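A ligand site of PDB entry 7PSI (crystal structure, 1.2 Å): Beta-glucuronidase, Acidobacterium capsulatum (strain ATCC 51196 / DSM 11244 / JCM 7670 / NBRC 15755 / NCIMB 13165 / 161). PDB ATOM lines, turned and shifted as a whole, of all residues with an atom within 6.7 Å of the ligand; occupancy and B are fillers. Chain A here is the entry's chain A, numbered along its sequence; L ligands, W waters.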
ATOM      1  N   GLU A  45      11.777  11.560 -15.278  1.00  0.00           N
ATOM      2  CA  GLU A  45      10.552  10.789 -15.086  1.00  0.00           C
ATOM      3  C   GLU A  45      10.792   9.308 -15.314  1.00  0.00           C
ATOM      4  O   GLU A  45      11.355   8.933 -16.344  1.00  0.00           O
ATOM      5  CB  GLU A  45       9.528  11.313 -16.077  1.00  0.00           C
ATOM      6  CG  GLU A  45       9.060  12.698 -15.749  1.00  0.00           C
ATOM      7  CD  GLU A  45       8.286  12.848 -14.456  1.00  0.00           C
ATOM      8  OE1 GLU A  45       7.772  11.839 -13.939  1.00  0.00           O
ATOM      9  OE2 GLU A  45       8.135  14.012 -14.023  1.00  0.00           O
ATOM     10  N   ARG A  76      18.775  10.306 -10.995  1.00  0.00           N
ATOM     11  CA  ARG A  76      17.566   9.898 -10.262  1.00  0.00           C
ATOM     12  C   ARG A  76      16.451   9.730 -11.265  1.00  0.00           C
ATOM     13  O   ARG A  76      16.202  10.608 -12.085  1.00  0.00           O
ATOM     14  CB  ARG A  76      17.248  10.898  -9.144  1.00  0.00           C
ATOM     15  CG  ARG A  76      15.978  10.584  -8.406  1.00  0.00           C
ATOM     16  CD  ARG A  76      14.765  11.340  -8.880  1.00  0.00           C
ATOM     17  NE  ARG A  76      13.564  11.039  -8.133  1.00  0.00           N
ATOM     18  CZ  ARG A  76      12.473  11.796  -8.153  1.00  0.00           C
ATOM     19  NH1 ARG A  76      12.428  12.872  -8.921  1.00  0.00           N
ATOM     20  NH2 ARG A  76      11.393  11.418  -7.455  1.00  0.00           N
ATOM     21  N   GLY A  78      12.353   8.921 -11.266  1.00  0.00           N
ATOM     22  CA  GLY A  78      11.188   8.888 -10.389  1.00  0.00           C
ATOM     23  C   GLY A  78      10.117   9.816 -10.858  1.00  0.00           C
ATOM     24  O   GLY A  78       9.659   9.684 -12.009  1.00  0.00           O
ATOM     25  N   GLY A  79       9.730  10.768 -10.038  1.00  0.00           N
ATOM     26  CA  GLY A  79       8.751  11.755 -10.465  1.00  0.00           C
ATOM     27  C   GLY A  79       7.355  11.258 -10.402  1.00  0.00           C
ATOM     28  O   GLY A  79       7.087  10.084 -10.043  1.00  0.00           O
ATOM     29  N   ASN A  80       6.450  12.101 -10.802  1.00  0.00           N
ATOM     30  CA  ASN A  80       5.013  11.790 -10.737  1.00  0.00           C
ATOM     31  C   ASN A  80       4.699  10.583 -11.605  1.00  0.00           C
ATOM     32  O   ASN A  80       3.790   9.779 -11.291  1.00  0.00           O
ATOM     33  CB  ASN A  80       4.176  12.949 -11.268  1.00  0.00           C
ATOM     34  CG  ASN A  80       4.126  14.121 -10.334  1.00  0.00           C
ATOM     35  OD1 ASN A  80       4.501  14.012  -9.162  1.00  0.00           O
ATOM     36  ND2 ASN A  80       3.613  15.242 -10.855  1.00  0.00           N
ATOM     37  N   THR A  81       5.429  10.361 -12.680  1.00  0.00           N
ATOM     38  CA  THR A  81       5.146   9.224 -13.549  1.00  0.00           C
ATOM     39  C   THR A  81       5.529   7.918 -12.887  1.00  0.00           C
ATOM     40  O   THR A  81       5.101   6.888 -13.400  1.00  0.00           O
ATOM     41  CB  THR A  81       5.823   9.328 -14.901  1.00  0.00           C
ATOM     42  OG1 THR A  81       7.254   9.317 -14.746  1.00  0.00           O
ATOM     43  CG2 THR A  81       5.328  10.523 -15.661  1.00  0.00           C
ATOM     44  N   GLY A 103       8.948  14.119 -20.857  1.00  0.00           N
ATOM     45  CA  GLY A 103       9.396  15.313 -20.162  1.00  0.00           C
ATOM     46  C   GLY A 103       8.819  15.338 -18.761  1.00  0.00           C
ATOM     47  O   GLY A 103       7.980  14.519 -18.407  1.00  0.00           O
ATOM     48  N   PRO A 104       9.170  16.367 -17.990  1.00  0.00           N
ATOM     49  CA  PRO A 104       8.613  16.525 -16.650  1.00  0.00           C
ATOM     50  C   PRO A 104       7.097  16.456 -16.701  1.00  0.00           C
ATOM     51  O   PRO A 104       6.453  17.118 -17.527  1.00  0.00           O
ATOM     52  CB  PRO A 104       9.084  17.924 -16.258  1.00  0.00           C
ATOM     53  CG  PRO A 104      10.382  18.054 -16.954  1.00  0.00           C
ATOM     54  CD  PRO A 104      10.155  17.433 -18.306  1.00  0.00           C
ATOM     55  N   ASP A 105       6.515  15.718 -15.764  1.00  0.00           N
ATOM     56  CA  ASP A 105       5.061  15.598 -15.605  1.00  0.00           C
ATOM     57  C   ASP A 105       4.483  16.964 -15.291  1.00  0.00           C
ATOM     58  O   ASP A 105       5.029  17.699 -14.441  1.00  0.00           O
ATOM     59  CB  ASP A 105       4.742  14.604 -14.493  1.00  0.00           C
ATOM     60  CG  ASP A 105       3.240  14.354 -14.459  1.00  0.00           C
ATOM     61  OD1 ASP A 105       2.746  13.681 -15.410  1.00  0.00           O
ATOM     62  OD2 ASP A 105       2.592  14.922 -13.546  1.00  0.00           O
ATOM     63  N   LYS A 106       3.369  17.336 -15.938  1.00  0.00           N
ATOM     64  CA  LYS A 106       2.850  18.710 -15.760  1.00  0.00           C
ATOM     65  C   LYS A 106       1.778  18.770 -14.663  1.00  0.00           C
ATOM     66  O   LYS A 106       1.258  19.902 -14.470  1.00  0.00           O
ATOM     67  CB  LYS A 106       2.398  19.279 -17.096  1.00  0.00           C
ATOM     68  CG  LYS A 106       3.483  19.320 -18.148  1.00  0.00           C
ATOM     69  CD  LYS A 106       3.061  20.220 -19.284  1.00  0.00           C
ATOM     70  CE  LYS A 106       3.178  19.579 -20.638  1.00  0.00           C
ATOM     71  NZ  LYS A 106       4.591  19.345 -20.986  1.00  0.00           N
ATOM     72  N   GLY A 107       1.504  17.661 -13.958  1.00  0.00           N
ATOM     73  CA  GLY A 107       0.739  17.621 -12.693  1.00  0.00           C
ATOM     74  C   GLY A 107      -0.746  17.938 -12.859  1.00  0.00           C
ATOM     75  O   GLY A 107      -1.422  18.079 -11.806  1.00  0.00           O
ATOM     76  N   ASN A 172       7.016   8.717  -4.997  1.00  0.00           N
ATOM     77  CA  ASN A 172       7.429  10.121  -5.227  1.00  0.00           C
ATOM     78  C   ASN A 172       6.375  10.994  -4.573  1.00  0.00           C
ATOM     79  O   ASN A 172       5.182  10.808  -4.834  1.00  0.00           O
ATOM     80  CB  ASN A 172       7.505  10.356  -6.704  1.00  0.00           C
ATOM     81  CG  ASN A 172       7.649  11.817  -7.011  1.00  0.00           C
ATOM     82  OD1 ASN A 172       8.745  12.370  -6.966  1.00  0.00           O
ATOM     83  ND2 ASN A 172       6.576  12.424  -7.467  1.00  0.00           N
ATOM     84  N   GLU A 173       6.800  11.921  -3.722  1.00  0.00           N
ATOM     85  CA  GLU A 173       5.890  12.916  -3.127  1.00  0.00           C
ATOM     86  C   GLU A 173       4.603  12.270  -2.633  1.00  0.00           C
ATOM     87  O   GLU A 173       3.482  12.617  -3.019  1.00  0.00           O
ATOM     88  CB  GLU A 173       5.573  14.019  -4.126  1.00  0.00           C
ATOM     89  CG  GLU A 173       6.842  14.742  -4.589  1.00  0.00           C
ATOM     90  CD  GLU A 173       6.694  16.052  -5.336  1.00  0.00           C
ATOM     91  OE1 GLU A 173       5.606  16.341  -5.844  1.00  0.00           O
ATOM     92  OE2 GLU A 173       7.711  16.779  -5.427  1.00  0.00           O
ATOM     93  N   LEU A 176       1.541  14.212  -1.669  1.00  0.00           N
ATOM     94  CA  LEU A 176       0.686  14.801  -2.722  1.00  0.00           C
ATOM     95  C   LEU A 176      -0.039  13.730  -3.509  1.00  0.00           C
ATOM     96  O   LEU A 176      -0.668  14.059  -4.543  1.00  0.00           O
ATOM     97  CB  LEU A 176       1.510  15.651  -3.675  1.00  0.00           C
ATOM     98  CG  LEU A 176       2.260  16.777  -2.984  1.00  0.00           C
ATOM     99  CD1 LEU A 176       3.041  17.602  -4.016  1.00  0.00           C
ATOM    100  CD2 LEU A 176       1.304  17.680  -2.235  1.00  0.00           C
ATOM    101  N   ASP A 216      11.256  11.460  -0.391  1.00  0.00           N
ATOM    102  CA  ASP A 216      11.128  11.953  -1.776  1.00  0.00           C
ATOM    103  C   ASP A 216      10.038  12.989  -1.861  1.00  0.00           C
ATOM    104  O   ASP A 216       9.209  12.989  -2.787  1.00  0.00           O
ATOM    105  CB  ASP A 216      10.948  10.779  -2.722  1.00  0.00           C
ATOM    106  CG  ASP A 216      11.490  10.951  -4.126  1.00  0.00           C
ATOM    107  OD1 ASP A 216      12.457  11.749  -4.266  1.00  0.00           O
ATOM    108  OD2 ASP A 216      11.012  10.183  -5.009  1.00  0.00           O
ATOM    109  N   HIS A 241      12.801  17.420  -1.933  1.00  0.00           N
ATOM    110  CA  HIS A 241      12.507  18.140  -3.185  1.00  0.00           C
ATOM    111  C   HIS A 241      12.497  19.627  -2.898  1.00  0.00           C
ATOM    112  O   HIS A 241      12.153  20.026  -1.749  1.00  0.00           O
ATOM    113  CB  HIS A 241      11.175  17.729  -3.791  1.00  0.00           C
ATOM    114  CG  HIS A 241      11.183  16.306  -4.213  1.00  0.00           C
ATOM    115  ND1 HIS A 241      10.085  15.748  -4.861  1.00  0.00           N
ATOM    116  CD2 HIS A 241      12.121  15.321  -4.147  1.00  0.00           C
ATOM    117  CE1 HIS A 241      10.353  14.465  -5.133  1.00  0.00           C
ATOM    118  NE2 HIS A 241      11.558  14.182  -4.704  1.00  0.00           N
ATOM    119  N   TYR A 243      11.436  23.372  -5.154  1.00  0.00           N
ATOM    120  CA  TYR A 243      11.184  24.261  -6.298  1.00  0.00           C
ATOM    121  C   TYR A 243      11.175  25.672  -5.793  1.00  0.00           C
ATOM    122  O   TYR A 243      10.664  25.954  -4.703  1.00  0.00           O
ATOM    123  CB  TYR A 243       9.876  23.903  -6.999  1.00  0.00           C
ATOM    124  CG  TYR A 243      10.064  22.711  -7.902  1.00  0.00           C
ATOM    125  CD1 TYR A 243      10.326  21.455  -7.387  1.00  0.00           C
ATOM    126  CD2 TYR A 243      10.121  22.858  -9.276  1.00  0.00           C
ATOM    127  CE1 TYR A 243      10.627  20.382  -8.210  1.00  0.00           C
ATOM    128  CE2 TYR A 243      10.414  21.798 -10.116  1.00  0.00           C
ATOM    129  CZ  TYR A 243      10.651  20.557  -9.596  1.00  0.00           C
ATOM    130  OH  TYR A 243      10.988  19.525 -10.421  1.00  0.00           O
ATOM    131  N   GLU A 287      14.906  16.087  -6.316  1.00  0.00           N
ATOM    132  CA  GLU A 287      14.134  16.691  -7.413  1.00  0.00           C
ATOM    133  C   GLU A 287      14.079  18.175  -7.163  1.00  0.00           C
ATOM    134  O   GLU A 287      13.522  18.598  -6.133  1.00  0.00           O
ATOM    135  CB  GLU A 287      12.736  16.098  -7.534  1.00  0.00           C
ATOM    136  CG  GLU A 287      12.021  16.456  -8.779  1.00  0.00           C
ATOM    137  CD  GLU A 287      10.563  16.086  -8.697  1.00  0.00           C
ATOM    138  OE1 GLU A 287      10.274  14.926  -8.364  1.00  0.00           O
ATOM    139  OE2 GLU A 287       9.724  16.958  -9.091  1.00  0.00           O
ATOM    140  N   ASN A 289      13.833  22.113  -9.381  1.00  0.00           N
ATOM    141  CA  ASN A 289      14.005  23.046 -10.505  1.00  0.00           C
ATOM    142  C   ASN A 289      13.328  24.329 -10.145  1.00  0.00           C
ATOM    143  O   ASN A 289      12.875  24.534  -9.008  1.00  0.00           O
ATOM    144  CB  ASN A 289      13.623  22.451 -11.875  1.00  0.00           C
ATOM    145  CG  ASN A 289      14.716  22.792 -12.851  1.00  0.00           C
ATOM    146  OD1 ASN A 289      15.076  23.974 -12.919  1.00  0.00           O
ATOM    147  ND2 ASN A 289      15.246  21.828 -13.582  1.00  0.00           N
ATOM    148  N   CYS A 291      10.612  26.171 -11.445  1.00  0.00           N
ATOM    149  CA  CYS A 291       9.151  26.347 -11.486  1.00  0.00           C
ATOM    150  C   CYS A 291       8.524  24.996 -11.745  1.00  0.00           C
ATOM    151  O   CYS A 291       9.125  24.180 -12.452  1.00  0.00           O
ATOM    152  CB  CYS A 291       8.758  27.305 -12.595  1.00  0.00           C
ATOM    153  SG  CYS A 291       9.414  28.973 -12.382  1.00  0.00           S
ATOM    154  N   TYR A 292       7.284  24.829 -11.280  1.00  0.00           N
ATOM    155  CA  TYR A 292       6.520  23.582 -11.413  1.00  0.00           C
ATOM    156  C   TYR A 292       6.016  23.363 -12.811  1.00  0.00           C
ATOM    157  O   TYR A 292       6.038  24.205 -13.710  1.00  0.00           O
ATOM    158  CB  TYR A 292       5.340  23.646 -10.440  1.00  0.00           C
ATOM    159  CG  TYR A 292       5.770  23.466  -9.034  1.00  0.00           C
ATOM    160  CD1 TYR A 292       5.675  24.492  -8.112  1.00  0.00           C
ATOM    161  CD2 TYR A 292       6.238  22.231  -8.620  1.00  0.00           C
ATOM    162  CE1 TYR A 292       6.007  24.278  -6.791  1.00  0.00           C
ATOM    163  CE2 TYR A 292       6.637  22.017  -7.317  1.00  0.00           C
ATOM    164  CZ  TYR A 292       6.478  23.033  -6.392  1.00  0.00           C
ATOM    165  OH  TYR A 292       6.862  22.801  -5.109  1.00  0.00           O
ATOM    166  N   GLN A 293       5.456  22.162 -12.958  1.00  0.00           N
ATOM    167  CA  GLN A 293       4.745  21.751 -14.166  1.00  0.00           C
ATOM    168  C   GLN A 293       5.689  21.746 -15.355  1.00  0.00           C
ATOM    169  O   GLN A 293       5.250  22.040 -16.461  1.00  0.00           O
ATOM    170  CB  GLN A 293       3.512  22.638 -14.388  1.00  0.00           C
ATOM    171  CG  GLN A 293       2.553  22.559 -13.193  1.00  0.00           C
ATOM    172  CD  GLN A 293       1.153  23.021 -13.488  1.00  0.00           C
ATOM    173  OE1 GLN A 293       0.704  24.064 -12.992  1.00  0.00           O
ATOM    174  NE2 GLN A 293       0.417  22.247 -14.277  1.00  0.00           N
ATOM    175  N   GLY A 294       6.953  21.430 -15.166  1.00  0.00           N
ATOM    176  CA  GLY A 294       7.931  21.365 -16.248  1.00  0.00           C
ATOM    177  C   GLY A 294       8.555  22.732 -16.495  1.00  0.00           C
ATOM    178  O   GLY A 294       9.481  22.802 -17.313  1.00  0.00           O
ATOM    179  N   GLY A 295       8.154  23.759 -15.730  1.00  0.00           N
ATOM    180  CA  GLY A 295       8.780  25.063 -15.786  1.00  0.00           C
ATOM    181  C   GLY A 295       7.879  26.097 -16.375  1.00  0.00           C
ATOM    182  O   GLY A 295       6.864  25.776 -16.981  1.00  0.00           O
ATOM    183  N   HIS A 327      15.514  18.273 -12.070  1.00  0.00           N
ATOM    184  CA  HIS A 327      14.501  17.552 -12.861  1.00  0.00           C
ATOM    185  C   HIS A 327      14.481  18.078 -14.281  1.00  0.00           C
ATOM    186  O   HIS A 327      14.875  19.213 -14.553  1.00  0.00           O
ATOM    187  CB  HIS A 327      13.141  17.626 -12.198  1.00  0.00           C
ATOM    188  CG  HIS A 327      12.220  16.535 -12.566  1.00  0.00           C
ATOM    189  ND1 HIS A 327      12.497  15.210 -12.343  1.00  0.00           N
ATOM    190  CD2 HIS A 327      11.013  16.578 -13.209  1.00  0.00           C
ATOM    191  CE1 HIS A 327      11.494  14.498 -12.780  1.00  0.00           C
ATOM    192  NE2 HIS A 327      10.548  15.304 -13.317  1.00  0.00           N
ATOM    193  N   TYR A 334      12.254  23.679 -18.026  1.00  0.00           N
ATOM    194  CA  TYR A 334      13.395  23.762 -17.103  1.00  0.00           C
ATOM    195  C   TYR A 334      14.464  22.705 -17.334  1.00  0.00           C
ATOM    196  O   TYR A 334      15.416  22.682 -16.543  1.00  0.00           O
ATOM    197  CB  TYR A 334      13.004  23.798 -15.643  1.00  0.00           C
ATOM    198  CG  TYR A 334      12.212  22.650 -15.135  1.00  0.00           C
ATOM    199  CD1 TYR A 334      12.593  21.330 -15.276  1.00  0.00           C
ATOM    200  CD2 TYR A 334      11.081  22.867 -14.366  1.00  0.00           C
ATOM    201  CE1 TYR A 334      11.886  20.299 -14.701  1.00  0.00           C
ATOM    202  CE2 TYR A 334      10.374  21.865 -13.768  1.00  0.00           C
ATOM    203  CZ  TYR A 334      10.779  20.567 -13.908  1.00  0.00           C
ATOM    204  OH  TYR A 334      10.129  19.550 -13.281  1.00  0.00           O
HETATM  205  C1  LIG L   1       7.671  15.827 -11.182  1.00  0.00           C
HETATM  206  C2  LIG L   1       7.787  18.342 -11.119  1.00  0.00           C
HETATM  207  C3  LIG L   1       7.194  19.587 -11.699  1.00  0.00           C
HETATM  208  O1  LIG L   1       6.993  14.694 -11.742  1.00  0.00           O
HETATM  209  O2  LIG L   1       7.457  17.086 -13.199  1.00  0.00           O
HETATM  210  C4  LIG L   1       8.270  16.960  -9.108  1.00  0.00           C
HETATM  211  C5  LIG L   1       7.422  15.843  -9.670  1.00  0.00           C
HETATM  212  C6  LIG L   1       7.147  17.113 -11.784  1.00  0.00           C
HETATM  213  C7  LIG L   1       7.731  18.278  -9.588  1.00  0.00           C
HETATM  214  O3  LIG L   1       7.736  14.602  -9.070  1.00  0.00           O
HETATM  215  O4  LIG L   1       7.849  20.219 -12.548  1.00  0.00           O
HETATM  216  O5  LIG L   1       6.073  19.927 -11.345  1.00  0.00           O
HETATM  217  O6  LIG L   1       6.362  18.463  -9.173  1.00  0.00           O
HETATM  218  O   HOH W   1       5.042  18.673  -6.822  1.00  0.00           O
HETATM  219  O   HOH W   2       2.998  17.658  -9.201  1.00  0.00           O
HETATM  220  O   HOH W   3       3.644  18.542 -12.026  1.00  0.00           O
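The side-chain carboxylate (OE2) of Glu 287 is covalently linked to a carbon (C4) of the ligand, 1.5 Å away.
OH of Tyr 334 is in hydrogen-bond range of O4 of the ligand (2.5 Å).
An oxygen (O1) of the ligand is in hydrogen-bond range of the side-chain carboxylate (OE2) of Glu 45 (2.6 Å).
N of Asp 105 lies within hydrogen-bond range of O2 of the ligand, 3.1 Å away.
An oxygen (O2) of the ligand is in hydrogen-bond range of the backbone carbonyl oxygen (O) of Asp 105 (2.8 Å).
O1 of the ligand lies within hydrogen-bond range of N of Asn 80.
An oxygen (O3) of the ligand lies within hydrogen-bond range of the side-chain amide oxygen (OD1) of Asn 80 (3.3 Å).
The backbone NH (N) of Gln 293 lies within hydrogen-bond range of an oxygen (O5) of the ligand (2.8 Å).
The side-chain amide nitrogen (ND2) of Asn 172 sits at hydrogen-bond distance from an oxygen (O3) of the ligand (2.9 Å).
O4 of the ligand is in hydrogen-bond range of N of Gly 294, 3.0 Å away.
The side-chain carboxylate (OE2) of Glu 287 sits at hydrogen-bond distance from the side-chain hydroxyl (OH) of Tyr 243 (3.2 Å).
The side-chain hydroxyl (OH) of Tyr 334 lies within hydrogen-bond range of the side-chain hydroxyl (OH) of Tyr 243 (3.0 Å).
OE2 of Glu 45 is in hydrogen-bond range of N of Asp 105 (2.9 Å).
The side-chain carboxylate of Glu 45 lies within hydrogen-bond range of the side-chain hydroxyl of Thr 81 (2.7 Å).
OD2 of Asp 105 is in hydrogen-bond range of N of Gly 107, at 3.0 Å.
The side-chain amide nitrogen (ND2) of Asn 172 sits at hydrogen-bond distance from the side-chain amide oxygen (OD1) of Asn 80, at 3.1 Å.
The side-chain amide oxygen (OD1) of Asn 172 lies within hydrogen-bond range of the guanidinium group (NH2) of Arg 76, at 2.9 Å.
OE2 of Glu 173 lies within hydrogen-bond range of ND1 of His 241, at 2.6 Å.
CA of Gly 79 touches O3 of the ligand, at 3.3 Å.
CB of Pro 104 touches O2 of the ligand (3.6 Å).
Glu 173 touches the ligand.
Tyr 243 touches the ligand.
CD2 of Tyr 292 touches O5 of the ligand, at 3.6 Å.
His 327 touches the ligand.
Within 4 Å of the ligand: Glu 45, Gly 79, Asn 80, Pro 104, Asp 105, Asn 172, Glu 173, Tyr 243, Glu 287, Tyr 292, Gln 293, Gly 294, His 327 and Tyr 334.
Water W1 lies within hydrogen-bond range of the side-chain carboxylate (OE1) of Glu 173 and an oxygen (O6) of the ligand.
Water W3 lies within hydrogen-bond range of O5 of the ligand, O of Asp 105 and N of Gly 107.
Water W2 bridges ND2 of Asn 80 (3.0 Å) and O6 of the ligand (3.5 Å).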
